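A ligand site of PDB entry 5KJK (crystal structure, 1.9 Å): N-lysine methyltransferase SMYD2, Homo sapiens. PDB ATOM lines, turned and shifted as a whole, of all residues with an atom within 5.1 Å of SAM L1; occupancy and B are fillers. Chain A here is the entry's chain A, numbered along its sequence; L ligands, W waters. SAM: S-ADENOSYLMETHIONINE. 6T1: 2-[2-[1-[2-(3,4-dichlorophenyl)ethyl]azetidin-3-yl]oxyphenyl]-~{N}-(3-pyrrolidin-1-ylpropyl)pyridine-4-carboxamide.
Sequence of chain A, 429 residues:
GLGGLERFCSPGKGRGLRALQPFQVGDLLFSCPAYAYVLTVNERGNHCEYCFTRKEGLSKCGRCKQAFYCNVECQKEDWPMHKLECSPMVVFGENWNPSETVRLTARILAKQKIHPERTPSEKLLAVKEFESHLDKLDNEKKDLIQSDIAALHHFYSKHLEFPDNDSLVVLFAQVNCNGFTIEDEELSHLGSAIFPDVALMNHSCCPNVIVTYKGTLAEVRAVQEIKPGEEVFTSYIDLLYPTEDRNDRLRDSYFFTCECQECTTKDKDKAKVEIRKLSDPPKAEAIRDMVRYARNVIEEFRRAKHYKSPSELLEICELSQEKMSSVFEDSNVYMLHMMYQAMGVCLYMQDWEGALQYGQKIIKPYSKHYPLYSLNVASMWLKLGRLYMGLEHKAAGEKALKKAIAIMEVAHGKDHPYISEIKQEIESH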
ATOM      1  N   GLY A  12     -17.444  26.152 -21.193  1.00  0.00           N
ATOM      2  CA  GLY A  12     -16.682  24.990 -20.753  1.00  0.00           C
ATOM      3  C   GLY A  12     -15.317  24.834 -21.399  1.00  0.00           C
ATOM      4  O   GLY A  12     -14.627  23.838 -21.149  1.00  0.00           O
ATOM      5  N   LYS A  13     -14.904  25.799 -22.264  1.00  0.00           N
ATOM      6  CA  LYS A  13     -13.613  25.750 -22.990  1.00  0.00           C
ATOM      7  C   LYS A  13     -12.859  27.084 -22.939  1.00  0.00           C
ATOM      8  O   LYS A  13     -11.992  27.317 -23.780  1.00  0.00           O
ATOM      9  CB  LYS A  13     -13.802  25.313 -24.470  1.00  0.00           C
ATOM     10  CG  LYS A  13     -14.507  23.961 -24.672  1.00  0.00           C
ATOM     11  CD  LYS A  13     -14.609  23.685 -26.174  1.00  0.00           C
ATOM     12  CE  LYS A  13     -15.542  22.551 -26.507  1.00  0.00           C
ATOM     13  NZ  LYS A  13     -16.913  22.791 -25.998  1.00  0.00           N
ATOM     14  N   GLY A  14     -13.191  27.925 -21.955  1.00  0.00           N
ATOM     15  CA  GLY A  14     -12.566  29.222 -21.736  1.00  0.00           C
ATOM     16  C   GLY A  14     -12.732  30.135 -22.931  1.00  0.00           C
ATOM     17  O   GLY A  14     -13.840  30.287 -23.429  1.00  0.00           O
ATOM     18  N   ARG A  15     -11.641  30.723 -23.415  1.00  0.00           N
ATOM     19  CA  ARG A  15     -11.715  31.596 -24.585  1.00  0.00           C
ATOM     20  C   ARG A  15     -11.463  30.773 -25.847  1.00  0.00           C
ATOM     21  O   ARG A  15     -10.685  29.821 -25.823  1.00  0.00           O
ATOM     22  CB  ARG A  15     -10.715  32.757 -24.495  1.00  0.00           C
ATOM     23  CG  ARG A  15     -10.963  33.664 -23.275  1.00  0.00           C
ATOM     24  CD  ARG A  15      -9.703  34.339 -22.769  1.00  0.00           C
ATOM     25  NE  ARG A  15      -8.592  33.401 -22.514  1.00  0.00           N
ATOM     26  CZ  ARG A  15      -7.436  33.751 -21.975  1.00  0.00           C
ATOM     27  NH1 ARG A  15      -6.480  32.845 -21.789  1.00  0.00           N
ATOM     28  NH2 ARG A  15      -7.209  35.015 -21.617  1.00  0.00           N
ATOM     29  N   GLY A  16     -12.115  31.121 -26.935  1.00  0.00           N
ATOM     30  CA  GLY A  16     -11.923  30.431 -28.197  1.00  0.00           C
ATOM     31  C   GLY A  16     -12.011  31.336 -29.402  1.00  0.00           C
ATOM     32  O   GLY A  16     -12.185  32.552 -29.272  1.00  0.00           O
ATOM     33  N   LEU A 125      -5.124  37.242 -29.011  1.00  0.00           N
ATOM     34  CA  LEU A 125      -4.734  36.738 -27.698  1.00  0.00           C
ATOM     35  C   LEU A 125      -3.293  37.126 -27.470  1.00  0.00           C
ATOM     36  O   LEU A 125      -2.468  36.962 -28.356  1.00  0.00           O
ATOM     37  CB  LEU A 125      -4.921  35.202 -27.625  1.00  0.00           C
ATOM     38  CG  LEU A 125      -4.579  34.485 -26.317  1.00  0.00           C
ATOM     39  CD1 LEU A 125      -5.564  34.872 -25.185  1.00  0.00           C
ATOM     40  CD2 LEU A 125      -4.477  32.938 -26.524  1.00  0.00           C
ATOM     41  N   GLU A 131      -3.367  31.037 -20.753  1.00  0.00           N
ATOM     42  CA  GLU A 131      -3.855  30.163 -19.691  1.00  0.00           C
ATOM     43  C   GLU A 131      -2.647  29.350 -19.216  1.00  0.00           C
ATOM     44  O   GLU A 131      -1.898  28.833 -20.029  1.00  0.00           O
ATOM     45  CB  GLU A 131      -4.939  29.220 -20.221  1.00  0.00           C
ATOM     46  CG  GLU A 131      -5.439  28.229 -19.188  1.00  0.00           C
ATOM     47  CD  GLU A 131      -6.790  27.639 -19.522  1.00  0.00           C
ATOM     48  OE1 GLU A 131      -7.668  27.639 -18.630  1.00  0.00           O
ATOM     49  OE2 GLU A 131      -6.977  27.173 -20.655  1.00  0.00           O
ATOM     50  N   HIS A 133      -2.887  27.063 -16.055  1.00  0.00           N
ATOM     51  CA  HIS A 133      -3.242  25.882 -15.231  1.00  0.00           C
ATOM     52  C   HIS A 133      -2.310  25.747 -14.009  1.00  0.00           C
ATOM     53  O   HIS A 133      -2.076  24.643 -13.512  1.00  0.00           O
ATOM     54  CB  HIS A 133      -3.306  24.588 -16.059  1.00  0.00           C
ATOM     55  CG  HIS A 133      -4.464  24.572 -16.988  1.00  0.00           C
ATOM     56  ND1 HIS A 133      -4.293  24.460 -18.347  1.00  0.00           N
ATOM     57  CD2 HIS A 133      -5.781  24.761 -16.721  1.00  0.00           C
ATOM     58  CE1 HIS A 133      -5.509  24.548 -18.856  1.00  0.00           C
ATOM     59  NE2 HIS A 133      -6.425  24.737 -17.916  1.00  0.00           N
ATOM     60  N   CYS A 177       1.380  24.985 -21.993  1.00  0.00           N
ATOM     61  CA  CYS A 177      -0.028  24.991 -22.374  1.00  0.00           C
ATOM     62  C   CYS A 177      -0.245  25.566 -23.779  1.00  0.00           C
ATOM     63  O   CYS A 177      -1.200  25.159 -24.445  1.00  0.00           O
ATOM     64  CB  CYS A 177      -0.873  25.722 -21.328  1.00  0.00           C
ATOM     65  SG  CYS A 177      -2.668  25.691 -21.622  1.00  0.00           S
ATOM     66  N   ASN A 178       0.593  26.529 -24.196  1.00  0.00           N
ATOM     67  CA  ASN A 178       0.400  27.224 -25.455  1.00  0.00           C
ATOM     68  C   ASN A 178       1.488  27.104 -26.520  1.00  0.00           C
ATOM     69  O   ASN A 178       1.251  27.575 -27.641  1.00  0.00           O
ATOM     70  CB  ASN A 178       0.154  28.691 -25.144  1.00  0.00           C
ATOM     71  CG  ASN A 178      -1.082  28.890 -24.271  1.00  0.00           C
ATOM     72  OD1 ASN A 178      -2.188  28.967 -24.765  1.00  0.00           O
ATOM     73  ND2 ASN A 178      -0.909  28.914 -22.951  1.00  0.00           N
ATOM     74  N   ALA A 199      -2.737  29.865 -30.661  1.00  0.00           N
ATOM     75  CA  ALA A 199      -2.987  29.212 -29.377  1.00  0.00           C
ATOM     76  C   ALA A 199      -4.386  29.562 -28.816  1.00  0.00           C
ATOM     77  O   ALA A 199      -4.831  28.871 -27.913  1.00  0.00           O
ATOM     78  CB  ALA A 199      -1.885  29.542 -28.374  1.00  0.00           C
ATOM     79  N   LEU A 200      -5.111  30.550 -29.426  1.00  0.00           N
ATOM     80  CA  LEU A 200      -6.484  30.843 -28.998  1.00  0.00           C
ATOM     81  C   LEU A 200      -7.400  29.678 -29.346  1.00  0.00           C
ATOM     82  O   LEU A 200      -8.397  29.461 -28.647  1.00  0.00           O
ATOM     83  CB  LEU A 200      -7.028  32.165 -29.627  1.00  0.00           C
ATOM     84  CG  LEU A 200      -8.480  32.595 -29.326  1.00  0.00           C
ATOM     85  CD1 LEU A 200      -8.760  32.668 -27.795  1.00  0.00           C
ATOM     86  CD2 LEU A 200      -8.799  33.922 -29.981  1.00  0.00           C
ATOM     87  N   MET A 201      -7.087  28.940 -30.423  1.00  0.00           N
ATOM     88  CA  MET A 201      -7.963  27.840 -30.854  1.00  0.00           C
ATOM     89  C   MET A 201      -7.997  26.672 -29.884  1.00  0.00           C
ATOM     90  O   MET A 201      -6.965  26.203 -29.429  1.00  0.00           O
ATOM     91  CB  MET A 201      -7.600  27.330 -32.245  1.00  0.00           C
ATOM     92  CG  MET A 201      -7.780  28.396 -33.323  1.00  0.00           C
ATOM     93  SD  MET A 201      -7.384  27.704 -34.958  1.00  0.00           S
ATOM     94  CE  MET A 201      -5.597  27.582 -34.888  1.00  0.00           C
ATOM     95  N   ASN A 202      -9.195  26.230 -29.579  1.00  0.00           N
ATOM     96  CA  ASN A 202      -9.476  25.076 -28.747  1.00  0.00           C
ATOM     97  C   ASN A 202      -9.305  23.785 -29.538  1.00  0.00           C
ATOM     98  O   ASN A 202      -9.138  23.802 -30.764  1.00  0.00           O
ATOM     99  CB  ASN A 202     -10.875  25.176 -28.130  1.00  0.00           C
ATOM    100  CG  ASN A 202     -10.876  26.140 -26.983  1.00  0.00           C
ATOM    101  OD1 ASN A 202      -9.929  26.230 -26.225  1.00  0.00           O
ATOM    102  ND2 ASN A 202     -11.937  26.919 -26.883  1.00  0.00           N
ATOM    103  N   HIS A 203      -9.284  22.662 -28.809  1.00  0.00           N
ATOM    104  CA  HIS A 203      -9.092  21.332 -29.367  1.00  0.00           C
ATOM    105  C   HIS A 203     -10.385  20.587 -29.707  1.00  0.00           C
ATOM    106  O   HIS A 203     -11.391  20.662 -28.994  1.00  0.00           O
ATOM    107  CB  HIS A 203      -8.323  20.444 -28.365  1.00  0.00           C
ATOM    108  CG  HIS A 203      -8.217  19.012 -28.825  1.00  0.00           C
ATOM    109  ND1 HIS A 203      -9.173  18.067 -28.464  1.00  0.00           N
ATOM    110  CD2 HIS A 203      -7.334  18.445 -29.660  1.00  0.00           C
ATOM    111  CE1 HIS A 203      -8.823  16.958 -29.102  1.00  0.00           C
ATOM    112  NE2 HIS A 203      -7.710  17.134 -29.814  1.00  0.00           N
ATOM    113  N   SER A 204     -10.300  19.763 -30.767  1.00  0.00           N
ATOM    114  CA  SER A 204     -11.302  18.765 -31.131  1.00  0.00           C
ATOM    115  C   SER A 204     -10.574  17.602 -31.786  1.00  0.00           C
ATOM    116  O   SER A 204      -9.587  17.823 -32.476  1.00  0.00           O
ATOM    117  CB  SER A 204     -12.351  19.311 -32.090  1.00  0.00           C
ATOM    118  OG  SER A 204     -13.232  18.260 -32.478  1.00  0.00           O
ATOM    119  N   PHE A 233     -11.742  24.737 -34.395  1.00  0.00           N
ATOM    120  CA  PHE A 233     -10.978  23.740 -33.646  1.00  0.00           C
ATOM    121  C   PHE A 233      -9.858  23.101 -34.441  1.00  0.00           C
ATOM    122  O   PHE A 233     -10.023  22.728 -35.601  1.00  0.00           O
ATOM    123  CB  PHE A 233     -11.888  22.603 -33.156  1.00  0.00           C
ATOM    124  CG  PHE A 233     -13.000  22.969 -32.205  1.00  0.00           C
ATOM    125  CD1 PHE A 233     -12.731  23.285 -30.876  1.00  0.00           C
ATOM    126  CD2 PHE A 233     -14.329  22.895 -32.603  1.00  0.00           C
ATOM    127  CE1 PHE A 233     -13.773  23.574 -29.973  1.00  0.00           C
ATOM    128  CE2 PHE A 233     -15.372  23.200 -31.707  1.00  0.00           C
ATOM    129  CZ  PHE A 233     -15.082  23.550 -30.409  1.00  0.00           C
ATOM    130  N   TYR A 236      -4.907  18.980 -30.938  1.00  0.00           N
ATOM    131  CA  TYR A 236      -3.701  19.207 -30.150  1.00  0.00           C
ATOM    132  C   TYR A 236      -2.821  17.943 -30.141  1.00  0.00           C
ATOM    133  O   TYR A 236      -1.704  17.998 -29.666  1.00  0.00           O
ATOM    134  CB  TYR A 236      -4.079  19.521 -28.693  1.00  0.00           C
ATOM    135  CG  TYR A 236      -4.708  20.858 -28.387  1.00  0.00           C
ATOM    136  CD1 TYR A 236      -5.100  21.730 -29.408  1.00  0.00           C
ATOM    137  CD2 TYR A 236      -4.942  21.251 -27.066  1.00  0.00           C
ATOM    138  CE1 TYR A 236      -5.706  22.952 -29.126  1.00  0.00           C
ATOM    139  CE2 TYR A 236      -5.521  22.479 -26.778  1.00  0.00           C
ATOM    140  CZ  TYR A 236      -5.933  23.318 -27.810  1.00  0.00           C
ATOM    141  OH  TYR A 236      -6.426  24.554 -27.486  1.00  0.00           O
ATOM    142  N   TYR A 254      -2.698  19.042 -21.192  1.00  0.00           N
ATOM    143  CA  TYR A 254      -3.559  20.221 -21.311  1.00  0.00           C
ATOM    144  C   TYR A 254      -4.645  20.345 -20.266  1.00  0.00           C
ATOM    145  O   TYR A 254      -5.449  21.273 -20.352  1.00  0.00           O
ATOM    146  CB  TYR A 254      -4.170  20.304 -22.745  1.00  0.00           C
ATOM    147  CG  TYR A 254      -3.089  20.461 -23.788  1.00  0.00           C
ATOM    148  CD1 TYR A 254      -2.398  21.667 -23.933  1.00  0.00           C
ATOM    149  CD2 TYR A 254      -2.685  19.377 -24.568  1.00  0.00           C
ATOM    150  CE1 TYR A 254      -1.352  21.789 -24.843  1.00  0.00           C
ATOM    151  CE2 TYR A 254      -1.642  19.494 -25.491  1.00  0.00           C
ATOM    152  CZ  TYR A 254      -0.964  20.698 -25.607  1.00  0.00           C
ATOM    153  OH  TYR A 254       0.071  20.822 -26.498  1.00  0.00           O
ATOM    154  N   PHE A 255      -4.658  19.460 -19.269  1.00  0.00           N
ATOM    155  CA  PHE A 255      -5.555  19.494 -18.112  1.00  0.00           C
ATOM    156  C   PHE A 255      -7.057  19.539 -18.437  1.00  0.00           C
ATOM    157  O   PHE A 255      -7.802  20.196 -17.725  1.00  0.00           O
ATOM    158  CB  PHE A 255      -5.169  20.665 -17.170  1.00  0.00           C
ATOM    159  CG  PHE A 255      -3.703  20.714 -16.839  1.00  0.00           C
ATOM    160  CD1 PHE A 255      -3.199  20.027 -15.738  1.00  0.00           C
ATOM    161  CD2 PHE A 255      -2.817  21.459 -17.610  1.00  0.00           C
ATOM    162  CE1 PHE A 255      -1.834  20.081 -15.422  1.00  0.00           C
ATOM    163  CE2 PHE A 255      -1.458  21.505 -17.297  1.00  0.00           C
ATOM    164  CZ  PHE A 255      -0.978  20.816 -16.220  1.00  0.00           C
ATOM    165  N   PHE A 256      -7.495  18.857 -19.482  1.00  0.00           N
ATOM    166  CA  PHE A 256      -8.926  18.809 -19.806  1.00  0.00           C
ATOM    167  C   PHE A 256      -9.265  17.490 -20.454  1.00  0.00           C
ATOM    168  O   PHE A 256      -8.368  16.799 -20.932  1.00  0.00           O
ATOM    169  CB  PHE A 256      -9.335  20.001 -20.735  1.00  0.00           C
ATOM    170  CG  PHE A 256      -8.992  19.822 -22.208  1.00  0.00           C
ATOM    171  CD1 PHE A 256      -9.916  19.247 -23.085  1.00  0.00           C
ATOM    172  CD2 PHE A 256      -7.763  20.233 -22.702  1.00  0.00           C
ATOM    173  CE1 PHE A 256      -9.593  19.057 -24.449  1.00  0.00           C
ATOM    174  CE2 PHE A 256      -7.451  20.062 -24.064  1.00  0.00           C
ATOM    175  CZ  PHE A 256      -8.371  19.477 -24.921  1.00  0.00           C
ATOM    176  N   THR A 257     -10.552  17.164 -20.488  1.00  0.00           N
ATOM    177  CA  THR A 257     -11.105  15.993 -21.156  1.00  0.00           C
ATOM    178  C   THR A 257     -11.971  16.509 -22.290  1.00  0.00           C
ATOM    179  O   THR A 257     -12.841  17.371 -22.090  1.00  0.00           O
ATOM    180  CB  THR A 257     -11.908  15.101 -20.198  1.00  0.00           C
ATOM    181  OG1 THR A 257     -11.021  14.616 -19.199  1.00  0.00           O
ATOM    182  CG2 THR A 257     -12.625  13.909 -20.906  1.00  0.00           C
ATOM    183  N   CYS A 258     -11.722  15.989 -23.472  1.00  0.00           N
ATOM    184  CA  CYS A 258     -12.446  16.333 -24.677  1.00  0.00           C
ATOM    185  C   CYS A 258     -13.786  15.653 -24.677  1.00  0.00           C
ATOM    186  O   CYS A 258     -13.896  14.481 -24.301  1.00  0.00           O
ATOM    187  CB  CYS A 258     -11.642  15.935 -25.922  1.00  0.00           C
ATOM    188  SG  CYS A 258     -12.399  16.505 -27.463  1.00  0.00           S
HETATM  189  N   SAM L   1      -9.307  28.100 -24.213  1.00  0.00           N
HETATM  190  CA  SAM L   1      -7.927  28.617 -24.120  1.00  0.00           C
HETATM  191  C   SAM L   1      -7.831  30.020 -23.386  1.00  0.00           C
HETATM  192  O   SAM L   1      -8.892  30.479 -22.894  1.00  0.00           O
HETATM  193  OXT SAM L   1      -6.708  30.556 -23.318  1.00  0.00           O
HETATM  194  CB  SAM L   1      -7.256  28.651 -25.514  1.00  0.00           C
HETATM  195  CG  SAM L   1      -6.609  27.322 -25.877  1.00  0.00           C
HETATM  196  SD  SAM L   1      -5.173  27.029 -24.811  1.00  0.00           S
HETATM  197  CE  SAM L   1      -3.898  26.677 -25.921  1.00  0.00           C
HETATM  198  C5' SAM L   1      -5.435  25.343 -24.286  1.00  0.00           C
HETATM  199  C4' SAM L   1      -6.403  25.202 -23.129  1.00  0.00           C
HETATM  200  O4' SAM L   1      -7.758  25.428 -23.576  1.00  0.00           O
HETATM  201  C3' SAM L   1      -6.439  23.810 -22.512  1.00  0.00           C
HETATM  202  O3' SAM L   1      -5.333  23.568 -21.661  1.00  0.00           O
HETATM  203  C2' SAM L   1      -7.830  23.770 -21.884  1.00  0.00           C
HETATM  204  O2' SAM L   1      -7.942  24.439 -20.636  1.00  0.00           O
HETATM  205  C1' SAM L   1      -8.656  24.526 -22.936  1.00  0.00           C
HETATM  206  N9  SAM L   1      -9.276  23.679 -23.954  1.00  0.00           N
HETATM  207  C8  SAM L   1      -8.890  23.517 -25.261  1.00  0.00           C
HETATM  208  N7  SAM L   1      -9.680  22.726 -25.949  1.00  0.00           N
HETATM  209  C5  SAM L   1     -10.641  22.321 -25.038  1.00  0.00           C
HETATM  210  C6  SAM L   1     -11.759  21.466 -25.138  1.00  0.00           C
HETATM  211  N6  SAM L   1     -12.154  20.889 -26.287  1.00  0.00           N
HETATM  212  N1  SAM L   1     -12.493  21.246 -24.025  1.00  0.00           N
HETATM  213  C2  SAM L   1     -12.133  21.859 -22.884  1.00  0.00           C
HETATM  214  N3  SAM L   1     -11.117  22.705 -22.677  1.00  0.00           N
HETATM  215  C4  SAM L   1     -10.406  22.905 -23.798  1.00  0.00           C
HETATM  216  C1  6T1 L   2       6.957  24.202 -26.474  1.00  0.00           C
HETATM  217  C2  6T1 L   2       7.121  24.154 -25.100  1.00  0.00           C
HETATM  218  C3  6T1 L   2       6.604  23.090 -24.367  1.00  0.00           C
HETATM  219  C7  6T1 L   2       4.992  21.060 -27.181  1.00  0.00           C
HETATM  220  C8  6T1 L   2       4.088  21.380 -28.201  1.00  0.00           C
HETATM  221  C9  6T1 L   2       3.436  20.354 -28.871  1.00  0.00           C
HETATM  222  C10 6T1 L   2       3.646  19.037 -28.458  1.00  0.00           C
HETATM  223  C11 6T1 L   2       4.547  18.807 -27.449  1.00  0.00           C
HETATM  224  C12 6T1 L   2       2.581  20.695 -30.044  1.00  0.00           C
HETATM  225  C13 6T1 L   2       0.443  20.315 -31.166  1.00  0.00           C
HETATM  226  C14 6T1 L   2      -0.593  21.223 -30.535  1.00  0.00           C
HETATM  227  C15 6T1 L   2      -0.022  22.462 -29.849  1.00  0.00           C
HETATM  228  C16 6T1 L   2      -1.829  23.009 -28.236  1.00  0.00           C
HETATM  229  C19 6T1 L   2      -0.454  24.711 -28.980  1.00  0.00           C
HETATM  230  C20 6T1 L   2       6.081  19.959 -23.802  1.00  0.00           C
HETATM  231  C21 6T1 L   2       5.485  18.555 -23.969  1.00  0.00           C
HETATM  232  C22 6T1 L   2       5.887  19.748 -22.303  1.00  0.00           C
HETATM  233  C24 6T1 L   2       3.962  17.918 -20.396  1.00  0.00           C
HETATM  234  C27 6T1 L   2       2.121  20.831 -18.760  1.00  0.00           C
HETATM  235  C30 6T1 L   2       4.627  19.622 -18.665  1.00  0.00           C
HETATM  236 CL2  6T1 L   2       2.746  22.702 -16.903  1.00  0.00          CL
HETATM  237  C28 6T1 L   2       3.083  21.295 -17.872  1.00  0.00           C
HETATM  238  C26 6T1 L   2       2.412  19.773 -19.593  1.00  0.00           C
HETATM  239  C29 6T1 L   2       4.329  20.668 -17.815  1.00  0.00           C
HETATM  240 CL1  6T1 L   2       5.525  21.157 -16.657  1.00  0.00          CL
HETATM  241  C25 6T1 L   2       3.668  19.145 -19.556  1.00  0.00           C
HETATM  242  C23 6T1 L   2       3.769  18.109 -21.897  1.00  0.00           C
HETATM  243  N4  6T1 L   2       4.921  18.695 -22.601  1.00  0.00           N
HETATM  244  O2  6T1 L   2       5.270  21.036 -24.373  1.00  0.00           O
HETATM  245  C4  6T1 L   2       5.904  22.082 -25.040  1.00  0.00           C
HETATM  246  C5  6T1 L   2       5.726  22.107 -26.432  1.00  0.00           C
HETATM  247  C6  6T1 L   2       6.270  23.195 -27.134  1.00  0.00           C
HETATM  248  N1  6T1 L   2       5.240  19.784 -26.815  1.00  0.00           N
HETATM  249  O1  6T1 L   2       2.879  21.629 -30.789  1.00  0.00           O
HETATM  250  N2  6T1 L   2       1.468  19.962 -30.198  1.00  0.00           N
HETATM  251  N3  6T1 L   2      -1.013  23.421 -29.385  1.00  0.00           N
HETATM  252  C18 6T1 L   2      -1.636  25.418 -28.355  1.00  0.00           C
HETATM  253  C17 6T1 L   2      -2.438  24.308 -27.739  1.00  0.00           C
HETATM  254  O   HOH W   1      -4.023  30.538 -23.491  1.00  0.00           O
HETATM  255  O   HOH W   2     -13.963  19.654 -28.864  1.00  0.00           O
HETATM  256  O   HOH W   3     -14.335  19.258 -23.284  1.00  0.00           O
HETATM  257  O   HOH W   4      -9.332  30.650 -19.684  1.00  0.00           O
HETATM  258  O   HOH W   5      -9.505  27.429 -21.472  1.00  0.00           O
HETATM  259  O   HOH W   6     -14.517  19.029 -26.354  1.00  0.00           O
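O2' of SAM L1 lies within hydrogen-bond range of OE2 of Glu 131, at 2.9 Å. O of Lys 13 is in hydrogen-bond range of N of SAM L1, 2.8 Å away. N6 of SAM L1 sits at hydrogen-bond distance from O of His 203 (2.8 Å). The guanidinium group (NH1) of Arg 15 lies within salt-bridge range of an oxygen (OXT) of SAM L1. The backbone carbonyl oxygen (O) of Tyr 254 lies within hydrogen-bond range of an oxygen (O3') of SAM L1 (2.6 Å). N of His 203 sits at hydrogen-bond distance from N7 of SAM L1, 2.9 Å away. O of SAM L1 is in hydrogen-bond range of N of Arg 15 (2.8 Å). A ring nitrogen (NE2) of His 133 lies close to an oxygen (O2') of SAM L1 (3.1 Å). A nitrogen (N) of SAM L1 sits at hydrogen-bond distance from the side-chain amide oxygen of Asn 202. The backbone carbonyl oxygen (O) of Arg 15 sits at hydrogen-bond distance from a nitrogen (N) of SAM L1 (2.7 Å). The side-chain sulfur (SG) of Cys 177 sits at hydrogen-bond distance from an oxygen (O3') of SAM L1.
The backbone carbonyl oxygen of Met 201 is in hydrogen-bond range of the side-chain hydroxyl of Tyr 236, 2.6 Å away. NE2 of His 133 lies within hydrogen-bond range of OE1 of Glu 131 (3.2 Å). The backbone carbonyl oxygen of Glu 131 sits at hydrogen-bond distance from the side-chain amide nitrogen of Asn 178. The backbone carbonyl oxygen (O) of Lys 13 lies within hydrogen-bond range of the side-chain amide nitrogen (ND2) of Asn 202 (3.1 Å). ND2 of Asn 202 lies within hydrogen-bond range of O of Arg 15. A ring nitrogen (ND1) of His 203 sits close to the side-chain sulfur of Cys 258, at 3.7 Å. O of Glu 131 lies close to SG of Cys 177 (3.6 Å).
The side-chain amide oxygen of Asn 178 lies close to a sulfur (SD) of SAM L1 (3.6 Å). O of Ala 199 sits close to SD of SAM L1 (3.6 Å). Residues that only touch SAM L1: Gly 12, Gly 14, Leu 200, Met 201, Tyr 236 and Phe 256. Hydrophobic or aromatic side chains that line SAM L1: His 133, His 203, Tyr 236, Tyr 254 and Phe 256. 16 residues have an atom within 4 Å of SAM L1: Gly 12, Lys 13, Gly 14, Arg 15, Glu 131, His 133, Cys 177, Asn 178, Ala 199, Leu 200, Met 201, Asn 202, His 203, Tyr 236, Tyr 254 and Phe 256. Along chain A the residues within 4 Å of SAM L1 span positions 12 to 256. The nearest printed residue that does not touch SAM L1 is Thr 257 (4.3 Å).
Water W1 lies within hydrogen-bond range of OXT of SAM L1 (2.7 Å), OD1 of Asn 178 (2.7 Å) and N of Glu 131 (2.9 Å). Water W3 bridges the backbone carbonyl oxygen of Thr 257 (2.7 Å) and a nitrogen (N1) of SAM L1 (2.8 Å). Water W5 lies within hydrogen-bond range of OE2 of Glu 131 (2.7 Å), N of SAM L1 (2.8 Å) and O of Lys 13 (3.4 Å). Water W2 lies within hydrogen-bond range of O of His 203 and N6 of SAM L1.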
